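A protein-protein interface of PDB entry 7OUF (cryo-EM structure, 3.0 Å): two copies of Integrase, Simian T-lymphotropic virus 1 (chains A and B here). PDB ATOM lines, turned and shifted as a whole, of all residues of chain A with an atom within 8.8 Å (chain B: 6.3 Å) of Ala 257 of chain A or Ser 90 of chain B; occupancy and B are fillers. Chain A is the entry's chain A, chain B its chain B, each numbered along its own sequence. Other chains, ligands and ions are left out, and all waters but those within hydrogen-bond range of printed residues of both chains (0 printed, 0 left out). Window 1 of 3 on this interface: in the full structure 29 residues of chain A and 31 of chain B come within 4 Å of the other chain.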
ATOM      1  N   GLN A 254       2.563 -19.600  21.950  1.00  0.00           N
ATOM      2  CA  GLN A 254       3.567 -20.102  21.029  1.00  0.00           C
ATOM      3  C   GLN A 254       3.851 -19.045  19.973  1.00  0.00           C
ATOM      4  O   GLN A 254       2.959 -18.298  19.566  1.00  0.00           O
ATOM      5  CB  GLN A 254       3.106 -21.404  20.363  1.00  0.00           C
ATOM      6  CG  GLN A 254       4.224 -22.253  19.794  1.00  0.00           C
ATOM      7  CD  GLN A 254       3.724 -23.572  19.238  1.00  0.00           C
ATOM      8  OE1 GLN A 254       2.609 -24.002  19.537  1.00  0.00           O
ATOM      9  NE2 GLN A 254       4.548 -24.224  18.429  1.00  0.00           N
ATOM     10  N   GLU A 255       5.106 -18.983  19.541  1.00  0.00           N
ATOM     11  CA  GLU A 255       5.550 -18.033  18.531  1.00  0.00           C
ATOM     12  C   GLU A 255       6.079 -18.800  17.331  1.00  0.00           C
ATOM     13  O   GLU A 255       6.949 -19.665  17.476  1.00  0.00           O
ATOM     14  CB  GLU A 255       6.633 -17.108  19.088  1.00  0.00           C
ATOM     15  CG  GLU A 255       6.121 -15.761  19.556  1.00  0.00           C
ATOM     16  CD  GLU A 255       7.237 -14.838  19.996  1.00  0.00           C
ATOM     17  OE1 GLU A 255       8.409 -15.263  19.956  1.00  0.00           O
ATOM     18  OE2 GLU A 255       6.946 -13.687  20.382  1.00  0.00           O
ATOM     19  N   ALA A 256       5.557 -18.482  16.151  1.00  0.00           N
ATOM     20  CA  ALA A 256       5.976 -19.104  14.907  1.00  0.00           C
ATOM     21  C   ALA A 256       6.183 -18.021  13.859  1.00  0.00           C
ATOM     22  O   ALA A 256       5.928 -16.839  14.097  1.00  0.00           O
ATOM     23  CB  ALA A 256       4.952 -20.137  14.427  1.00  0.00           C
ATOM     24  N   ALA A 257       6.655 -18.433  12.688  1.00  0.00           N
ATOM     25  CA  ALA A 257       6.791 -17.504  11.578  1.00  0.00           C
ATOM     26  C   ALA A 257       5.413 -17.126  11.052  1.00  0.00           C
ATOM     27  O   ALA A 257       4.591 -17.995  10.748  1.00  0.00           O
ATOM     28  CB  ALA A 257       7.631 -18.126  10.468  1.00  0.00           C
ATOM     29  N   GLY A 258       5.154 -15.825  10.960  1.00  0.00           N
ATOM     30  CA  GLY A 258       3.921 -15.336  10.387  1.00  0.00           C
ATOM     31  C   GLY A 258       2.773 -15.146  11.350  1.00  0.00           C
ATOM     32  O   GLY A 258       1.821 -14.436  11.008  1.00  0.00           O
ATOM     33  N   ALA A 259       2.820 -15.740  12.540  1.00  0.00           N
ATOM     34  CA  ALA A 259       1.712 -15.616  13.477  1.00  0.00           C
ATOM     35  C   ALA A 259       2.186 -15.960  14.880  1.00  0.00           C
ATOM     36  O   ALA A 259       3.263 -16.528  15.072  1.00  0.00           O
ATOM     37  CB  ALA A 259       0.537 -16.515  13.078  1.00  0.00           C
ATOM     38  N   ALA A 260       1.360 -15.602  15.860  1.00  0.00           N
ATOM     39  CA  ALA A 260       1.589 -15.957  17.253  1.00  0.00           C
ATOM     40  C   ALA A 260       0.280 -16.427  17.871  1.00  0.00           C
ATOM     41  O   ALA A 260      -0.804 -16.032  17.441  1.00  0.00           O
ATOM     42  CB  ALA A 260       2.163 -14.783  18.055  1.00  0.00           C
ATOM     43  N   TRP A 271      -4.478 -18.061  16.309  1.00  0.00           N
ATOM     44  CA  TRP A 271      -3.213 -17.652  15.711  1.00  0.00           C
ATOM     45  C   TRP A 271      -3.418 -16.305  15.025  1.00  0.00           C
ATOM     46  O   TRP A 271      -4.053 -16.228  13.970  1.00  0.00           O
ATOM     47  CB  TRP A 271      -2.716 -18.705  14.726  1.00  0.00           C
ATOM     48  CG  TRP A 271      -2.118 -19.910  15.382  1.00  0.00           C
ATOM     49  CD1 TRP A 271      -2.727 -21.107  15.604  1.00  0.00           C
ATOM     50  CD2 TRP A 271      -0.790 -20.036  15.900  1.00  0.00           C
ATOM     51  NE1 TRP A 271      -1.863 -21.971  16.227  1.00  0.00           N
ATOM     52  CE2 TRP A 271      -0.666 -21.336  16.422  1.00  0.00           C
ATOM     53  CE3 TRP A 271       0.307 -19.174  15.974  1.00  0.00           C
ATOM     54  CZ2 TRP A 271       0.508 -21.796  17.007  1.00  0.00           C
ATOM     55  CZ3 TRP A 271       1.471 -19.633  16.556  1.00  0.00           C
ATOM     56  CH2 TRP A 271       1.563 -20.931  17.065  1.00  0.00           C
ATOM     57  N   ILE A 272      -2.887 -15.251  15.624  1.00  0.00           N
ATOM     58  CA  ILE A 272      -3.028 -13.889  15.120  1.00  0.00           C
ATOM     59  C   ILE A 272      -1.780 -13.548  14.312  1.00  0.00           C
ATOM     60  O   ILE A 272      -0.665 -13.803  14.789  1.00  0.00           O
ATOM     61  CB  ILE A 272      -3.226 -12.879  16.264  1.00  0.00           C
ATOM     62  CG1 ILE A 272      -4.314 -13.363  17.225  1.00  0.00           C
ATOM     63  CG2 ILE A 272      -3.573 -11.507  15.712  1.00  0.00           C
ATOM     64  CD1 ILE A 272      -5.685 -13.460  16.602  1.00  0.00           C
ATOM     65  N   PRO A 273      -1.916 -12.990  13.113  1.00  0.00           N
ATOM     66  CA  PRO A 273      -0.735 -12.630  12.323  1.00  0.00           C
ATOM     67  C   PRO A 273       0.051 -11.495  12.960  1.00  0.00           C
ATOM     68  O   PRO A 273      -0.434 -10.771  13.830  1.00  0.00           O
ATOM     69  CB  PRO A 273      -1.325 -12.207  10.973  1.00  0.00           C
ATOM     70  CG  PRO A 273      -2.683 -12.827  10.939  1.00  0.00           C
ATOM     71  CD  PRO A 273      -3.162 -12.821  12.349  1.00  0.00           C
ATOM     72  N   TRP A 274       1.298 -11.349  12.504  1.00  0.00           N
ATOM     73  CA  TRP A 274       2.194 -10.351  13.081  1.00  0.00           C
ATOM     74  C   TRP A 274       1.700  -8.932  12.822  1.00  0.00           C
ATOM     75  O   TRP A 274       1.847  -8.055  13.680  1.00  0.00           O
ATOM     76  CB  TRP A 274       3.607 -10.528  12.530  1.00  0.00           C
ATOM     77  CG  TRP A 274       4.354 -11.677  13.131  1.00  0.00           C
ATOM     78  CD1 TRP A 274       4.818 -12.776  12.480  1.00  0.00           C
ATOM     79  CD2 TRP A 274       4.731 -11.835  14.503  1.00  0.00           C
ATOM     80  NE1 TRP A 274       5.454 -13.614  13.358  1.00  0.00           N
ATOM     81  CE2 TRP A 274       5.413 -13.060  14.608  1.00  0.00           C
ATOM     82  CE3 TRP A 274       4.554 -11.062  15.653  1.00  0.00           C
ATOM     83  CZ2 TRP A 274       5.921 -13.529  15.815  1.00  0.00           C
ATOM     84  CZ3 TRP A 274       5.058 -11.531  16.849  1.00  0.00           C
ATOM     85  CH2 TRP A 274       5.734 -12.752  16.921  1.00  0.00           C
ATOM     86  N   ARG B  58      -2.691 -20.636   7.616  1.00  0.00           N
ATOM     87  CA  ARG B  58      -1.403 -21.062   8.138  1.00  0.00           C
ATOM     88  C   ARG B  58      -1.544 -22.387   8.871  1.00  0.00           C
ATOM     89  O   ARG B  58      -2.561 -22.656   9.515  1.00  0.00           O
ATOM     90  CB  ARG B  58      -0.808 -20.012   9.078  1.00  0.00           C
ATOM     91  CG  ARG B  58      -0.515 -18.690   8.405  1.00  0.00           C
ATOM     92  CD  ARG B  58       0.682 -18.016   9.031  1.00  0.00           C
ATOM     93  NE  ARG B  58       1.127 -16.867   8.252  1.00  0.00           N
ATOM     94  CZ  ARG B  58       2.252 -16.826   7.552  1.00  0.00           C
ATOM     95  NH1 ARG B  58       3.077 -17.858   7.506  1.00  0.00           N
ATOM     96  NH2 ARG B  58       2.559 -15.720   6.885  1.00  0.00           N
ATOM     97  N   LEU B  61       1.163 -26.717  12.837  1.00  0.00           N
ATOM     98  CA  LEU B  61       2.399 -27.401  13.192  1.00  0.00           C
ATOM     99  C   LEU B  61       3.200 -27.627  11.916  1.00  0.00           C
ATOM    100  O   LEU B  61       2.649 -27.483  10.819  1.00  0.00           O
ATOM    101  CB  LEU B  61       2.096 -28.709  13.933  1.00  0.00           C
ATOM    102  CG  LEU B  61       1.205 -29.794  13.323  1.00  0.00           C
ATOM    103  CD1 LEU B  61       1.946 -30.696  12.365  1.00  0.00           C
ATOM    104  CD2 LEU B  61       0.634 -30.620  14.441  1.00  0.00           C
ATOM    105  N   PRO B  62       4.494 -27.942  12.002  1.00  0.00           N
ATOM    106  CA  PRO B  62       5.287 -28.128  10.781  1.00  0.00           C
ATOM    107  C   PRO B  62       4.741 -29.243   9.902  1.00  0.00           C
ATOM    108  O   PRO B  62       4.230 -30.253  10.387  1.00  0.00           O
ATOM    109  CB  PRO B  62       6.681 -28.471  11.315  1.00  0.00           C
ATOM    110  CG  PRO B  62       6.725 -27.846  12.651  1.00  0.00           C
ATOM    111  CD  PRO B  62       5.341 -27.968  13.208  1.00  0.00           C
ATOM    112  N   ASN B  63       4.863 -29.043   8.591  1.00  0.00           N
ATOM    113  CA  ASN B  63       4.383 -29.995   7.588  1.00  0.00           C
ATOM    114  C   ASN B  63       2.868 -30.166   7.654  1.00  0.00           C
ATOM    115  O   ASN B  63       2.344 -31.274   7.537  1.00  0.00           O
ATOM    116  CB  ASN B  63       5.086 -31.348   7.716  1.00  0.00           C
ATOM    117  CG  ASN B  63       6.533 -31.295   7.291  1.00  0.00           C
ATOM    118  OD1 ASN B  63       6.897 -30.552   6.384  1.00  0.00           O
ATOM    119  ND2 ASN B  63       7.368 -32.087   7.945  1.00  0.00           N
ATOM    120  N   ASP B  87       6.992 -23.707   3.908  1.00  0.00           N
ATOM    121  CA  ASP B  87       6.119 -24.175   4.973  1.00  0.00           C
ATOM    122  C   ASP B  87       5.482 -22.983   5.673  1.00  0.00           C
ATOM    123  O   ASP B  87       6.181 -22.068   6.117  1.00  0.00           O
ATOM    124  CB  ASP B  87       6.901 -25.025   5.973  1.00  0.00           C
ATOM    125  CG  ASP B  87       6.000 -25.835   6.879  1.00  0.00           C
ATOM    126  OD1 ASP B  87       5.473 -25.274   7.859  1.00  0.00           O
ATOM    127  OD2 ASP B  87       5.816 -27.038   6.608  1.00  0.00           O
ATOM    128  N   THR B  88       4.154 -23.002   5.779  1.00  0.00           N
ATOM    129  CA  THR B  88       3.422 -21.857   6.304  1.00  0.00           C
ATOM    130  C   THR B  88       3.534 -21.714   7.815  1.00  0.00           C
ATOM    131  O   THR B  88       3.059 -20.713   8.357  1.00  0.00           O
ATOM    132  CB  THR B  88       1.949 -21.948   5.904  1.00  0.00           C
ATOM    133  OG1 THR B  88       1.432 -23.232   6.264  1.00  0.00           O
ATOM    134  CG2 THR B  88       1.798 -21.753   4.407  1.00  0.00           C
ATOM    135  N   PHE B  89       4.135 -22.679   8.507  1.00  0.00           N
ATOM    136  CA  PHE B  89       4.327 -22.590   9.952  1.00  0.00           C
ATOM    137  C   PHE B  89       5.746 -22.167  10.309  1.00  0.00           C
ATOM    138  O   PHE B  89       5.944 -21.181  11.025  1.00  0.00           O
ATOM    139  CB  PHE B  89       3.992 -23.932  10.614  1.00  0.00           C
ATOM    140  CG  PHE B  89       4.197 -23.941  12.100  1.00  0.00           C
ATOM    141  CD1 PHE B  89       3.205 -23.493  12.948  1.00  0.00           C
ATOM    142  CD2 PHE B  89       5.383 -24.398  12.649  1.00  0.00           C
ATOM    143  CE1 PHE B  89       3.390 -23.501  14.312  1.00  0.00           C
ATOM    144  CE2 PHE B  89       5.572 -24.404  14.011  1.00  0.00           C
ATOM    145  CZ  PHE B  89       4.574 -23.956  14.843  1.00  0.00           C
ATOM    146  N   SER B  90       6.741 -22.904   9.825  1.00  0.00           N
ATOM    147  CA  SER B  90       8.131 -22.633  10.156  1.00  0.00           C
ATOM    148  C   SER B  90       8.803 -21.668   9.193  1.00  0.00           C
ATOM    149  O   SER B  90       9.811 -21.054   9.560  1.00  0.00           O
ATOM    150  CB  SER B  90       8.923 -23.941  10.188  1.00  0.00           C
ATOM    151  OG  SER B  90       8.910 -24.568   8.920  1.00  0.00           O
ATOM    152  N   GLY B  91       8.275 -21.513   7.983  1.00  0.00           N
ATOM    153  CA  GLY B  91       8.910 -20.688   6.982  1.00  0.00           C
ATOM    154  C   GLY B  91      10.026 -21.360   6.219  1.00  0.00           C
ATOM    155  O   GLY B  91      10.691 -20.694   5.420  1.00  0.00           O
ATOM    156  N   SER B  92      10.252 -22.653   6.441  1.00  0.00           N
ATOM    157  CA  SER B  92      11.325 -23.371   5.774  1.00  0.00           C
ATOM    158  C   SER B  92      11.080 -23.436   4.272  1.00  0.00           C
ATOM    159  O   SER B  92       9.949 -23.586   3.809  1.00  0.00           O
ATOM    160  CB  SER B  92      11.449 -24.778   6.345  1.00  0.00           C
ATOM    161  OG  SER B  92      11.642 -24.735   7.744  1.00  0.00           O
ATOM    162  N   LEU B 117      12.310 -31.752   3.623  1.00  0.00           N
ATOM    163  CA  LEU B 117      11.567 -31.252   4.775  1.00  0.00           C
ATOM    164  C   LEU B 117      10.666 -32.288   5.425  1.00  0.00           C
ATOM    165  O   LEU B 117      10.617 -32.367   6.653  1.00  0.00           O
ATOM    166  CB  LEU B 117      10.714 -30.045   4.364  1.00  0.00           C
ATOM    167  CG  LEU B 117      11.412 -28.787   3.840  1.00  0.00           C
ATOM    168  CD1 LEU B 117      10.396 -27.824   3.258  1.00  0.00           C
ATOM    169  CD2 LEU B 117      12.217 -28.108   4.933  1.00  0.00           C
ATOM    170  N   LEU B 201      14.653 -15.112  11.590  1.00  0.00           N
ATOM    171  CA  LEU B 201      13.368 -14.493  11.298  1.00  0.00           C
ATOM    172  C   LEU B 201      13.189 -13.219  12.116  1.00  0.00           C
ATOM    173  O   LEU B 201      13.628 -13.122  13.263  1.00  0.00           O
ATOM    174  CB  LEU B 201      12.232 -15.473  11.583  1.00  0.00           C
ATOM    175  CG  LEU B 201      12.017 -16.573  10.543  1.00  0.00           C
ATOM    176  CD1 LEU B 201      11.290 -17.747  11.157  1.00  0.00           C
ATOM    177  CD2 LEU B 201      11.249 -16.042   9.352  1.00  0.00           C
ATOM    178  N   CYS B 204       9.898 -13.511  15.335  1.00  0.00           N
ATOM    179  CA  CYS B 204      10.072 -14.522  16.369  1.00  0.00           C
ATOM    180  C   CYS B 204      11.516 -14.651  16.830  1.00  0.00           C
ATOM    181  O   CYS B 204      11.771 -15.360  17.809  1.00  0.00           O
ATOM    182  CB  CYS B 204       9.562 -15.880  15.881  1.00  0.00           C
ATOM    183  SG  CYS B 204      10.352 -16.500  14.392  1.00  0.00           S
ATOM    184  N   THR B 207      15.388 -19.083  13.900  1.00  0.00           N
ATOM    185  CA  THR B 207      15.722 -19.547  12.566  1.00  0.00           C
ATOM    186  C   THR B 207      14.635 -20.495  12.064  1.00  0.00           C
ATOM    187  O   THR B 207      13.956 -21.166  12.843  1.00  0.00           O
ATOM    188  CB  THR B 207      17.091 -20.233  12.584  1.00  0.00           C
ATOM    189  OG1 THR B 207      18.068 -19.322  13.098  1.00  0.00           O
ATOM    190  CG2 THR B 207      17.518 -20.631  11.196  1.00  0.00           C
ATOM    191  N   ARG B 208      14.458 -20.521  10.740  1.00  0.00           N
ATOM    192  CA  ARG B 208      13.447 -21.388  10.142  1.00  0.00           C
ATOM    193  C   ARG B 208      13.699 -22.851  10.483  1.00  0.00           C
ATOM    194  O   ARG B 208      12.761 -23.601  10.779  1.00  0.00           O
ATOM    195  CB  ARG B 208      13.424 -21.191   8.627  1.00  0.00           C
ATOM    196  CG  ARG B 208      12.970 -19.816   8.188  1.00  0.00           C
ATOM    197  CD  ARG B 208      13.402 -19.528   6.765  1.00  0.00           C
ATOM    198  NE  ARG B 208      12.616 -18.463   6.159  1.00  0.00           N
ATOM    199  CZ  ARG B 208      12.870 -17.170   6.301  1.00  0.00           C
ATOM    200  NH1 ARG B 208      13.891 -16.742   7.020  1.00  0.00           N
ATOM    201  NH2 ARG B 208      12.078 -16.286   5.705  1.00  0.00           N
ATOM    202  N   TRP B 209      14.964 -23.274  10.446  1.00  0.00           N
ATOM    203  CA  TRP B 209      15.300 -24.652  10.784  1.00  0.00           C
ATOM    204  C   TRP B 209      14.972 -24.961  12.240  1.00  0.00           C
ATOM    205  O   TRP B 209      14.514 -26.064  12.556  1.00  0.00           O
ATOM    206  CB  TRP B 209      16.775 -24.915  10.497  1.00  0.00           C
ATOM    207  CG  TRP B 209      17.062 -26.308  10.048  1.00  0.00           C
ATOM    208  CD1 TRP B 209      17.887 -27.210  10.652  1.00  0.00           C
ATOM    209  CD2 TRP B 209      16.526 -26.964   8.894  1.00  0.00           C
ATOM    210  NE1 TRP B 209      17.896 -28.386   9.947  1.00  0.00           N
ATOM    211  CE2 TRP B 209      17.069 -28.262   8.864  1.00  0.00           C
ATOM    212  CE3 TRP B 209      15.639 -26.579   7.883  1.00  0.00           C
ATOM    213  CZ2 TRP B 209      16.756 -29.176   7.863  1.00  0.00           C
ATOM    214  CZ3 TRP B 209      15.329 -27.488   6.894  1.00  0.00           C
ATOM    215  CH2 TRP B 209      15.886 -28.772   6.891  1.00  0.00           C
ATOM    216  N   LEU B 211      12.572 -23.622  14.073  1.00  0.00           N
ATOM    217  CA  LEU B 211      11.129 -23.813  14.167  1.00  0.00           C
ATOM    218  C   LEU B 211      10.695 -25.135  13.555  1.00  0.00           C
ATOM    219  O   LEU B 211       9.796 -25.794  14.088  1.00  0.00           O
ATOM    220  CB  LEU B 211      10.388 -22.664  13.486  1.00  0.00           C
ATOM    221  CG  LEU B 211      10.383 -21.305  14.179  1.00  0.00           C
ATOM    222  CD1 LEU B 211       9.697 -20.279  13.305  1.00  0.00           C
ATOM    223  CD2 LEU B 211       9.701 -21.399  15.526  1.00  0.00           C
ATOM    224  N   HIS B 212      11.308 -25.533  12.439  1.00  0.00           N
ATOM    225  CA  HIS B 212      10.884 -26.752  11.759  1.00  0.00           C
ATOM    226  C   HIS B 212      11.099 -27.983  12.629  1.00  0.00           C
ATOM    227  O   HIS B 212      10.259 -28.888  12.649  1.00  0.00           O
ATOM    228  CB  HIS B 212      11.630 -26.901  10.437  1.00  0.00           C
ATOM    229  CG  HIS B 212      10.950 -27.806   9.460  1.00  0.00           C
ATOM    230  ND1 HIS B 212       9.632 -27.646   9.090  1.00  0.00           N
ATOM    231  CD2 HIS B 212      11.403 -28.882   8.776  1.00  0.00           C
ATOM    232  CE1 HIS B 212       9.305 -28.581   8.219  1.00  0.00           C
ATOM    233  NE2 HIS B 212      10.361 -29.345   8.012  1.00  0.00           N
ATOM    234  N   HIS B 213      12.218 -28.042  13.346  1.00  0.00           N
ATOM    235  CA  HIS B 213      12.583 -29.222  14.116  1.00  0.00           C
ATOM    236  C   HIS B 213      12.417 -29.032  15.614  1.00  0.00           C
ATOM    237  O   HIS B 213      12.890 -29.871  16.386  1.00  0.00           O
ATOM    238  CB  HIS B 213      14.020 -29.632  13.798  1.00  0.00           C
ATOM    239  CG  HIS B 213      14.252 -29.921  12.350  1.00  0.00           C
ATOM    240  ND1 HIS B 213      13.708 -31.018  11.718  1.00  0.00           N
ATOM    241  CD2 HIS B 213      14.959 -29.255  11.408  1.00  0.00           C
ATOM    242  CE1 HIS B 213      14.074 -31.017  10.450  1.00  0.00           C
ATOM    243  NE2 HIS B 213      14.832 -29.957  10.236  1.00  0.00           N
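Of the 19 printed residues of chain B, 7 touch a printed residue of chain A. Hydrophobic or aromatic side chains of chain B that line the printed part of chain A: Phe 89, Leu 201 and Leu 211. Along chain B the printed residues that touch a printed residue of chain A span positions 58 to 211. Hydrophobic or aromatic side chains of chain A that line the printed part of chain B: Ala 256 and Ala 257. Among the printed residues, no Asp or Glu carboxylate lies within 4 Å of a Lys or Arg side-chain nitrogen of the other chain.
No position is printed for both chains. Of the 11 pairs that touch across the chains among the printed residues, none has its exchanged pair printed and touching as well.
The backbone carbonyl oxygen (O) of Gly 258 of chain A sits at hydrogen-bond distance from the backbone NH (N) of Trp 274 of chain A (3.5 Å). NH1 of Arg 58 of chain B sits at hydrogen-bond distance from O of Thr 88 of chain B. N of Phe 89 of chain B sits at hydrogen-bond distance from OD1 of Asp 87 of chain B (3.0 Å). The side-chain carboxylate (OD1) of Asp 87 of chain B is in hydrogen-bond range of the backbone NH (N) of Ser 90 of chain B (3.3 Å). OG of Ser 92 of chain B sits at hydrogen-bond distance from OG of Ser 90 of chain B. ND1 of His 212 of chain B sits at hydrogen-bond distance from OG of Ser 90 of chain B (3.2 Å).
Of the printed residues of chain B, Gln 254 of chain A touches Phe 89 (3.6 Å). Printed residues of chain B within 4 Å of Glu 255 of chain A: Cys 204 and Leu 211. Of chain B, only Arg 58 (3.6 Å), Thr 88 (3.9 Å), Phe 89 (3.3 Å), Ser 90 (3.8 Å), Leu 201 (3.7 Å) and Leu 211 (3.6 Å) come within 4 Å of Ala 257 of chain A. Ser 92 of chain B touches none of the printed residues of chain A. Printed residues of chain A within 4 Å of Cys 204 of chain B: Glu 255. The nearest printed residue of chain A that does not touch Phe 89 of chain B is Trp 271 of chain A (4.2 Å).
Among the printed residues, pairs that only touch across the chains: Ala 257 of chain A with Arg 58 of chain B (3.6 Å), Gln 254 of chain A with Phe 89 of chain B (3.6 Å), Ala 257 of chain A with Leu 211 of chain B (3.6 Å), Gly 258 of chain A with Arg 58 of chain B (3.6 Å), Ala 256 of chain A with Phe 89 of chain B (3.7 Å), Ala 257 of chain A with Leu 201 of chain B (3.7 Å), Ala 257 of chain A with Ser 90 of chain B (3.8 Å), Glu 255 of chain A with Leu 211 of chain B (3.8 Å), Ala 257 of chain A with Thr 88 of chain B (3.9 Å) and Glu 255 of chain A with Cys 204 of chain B (3.99 Å).
N of Ala 257 of chain A is in hydrogen-bond range of O of Phe 89 of chain B (3.3 Å).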
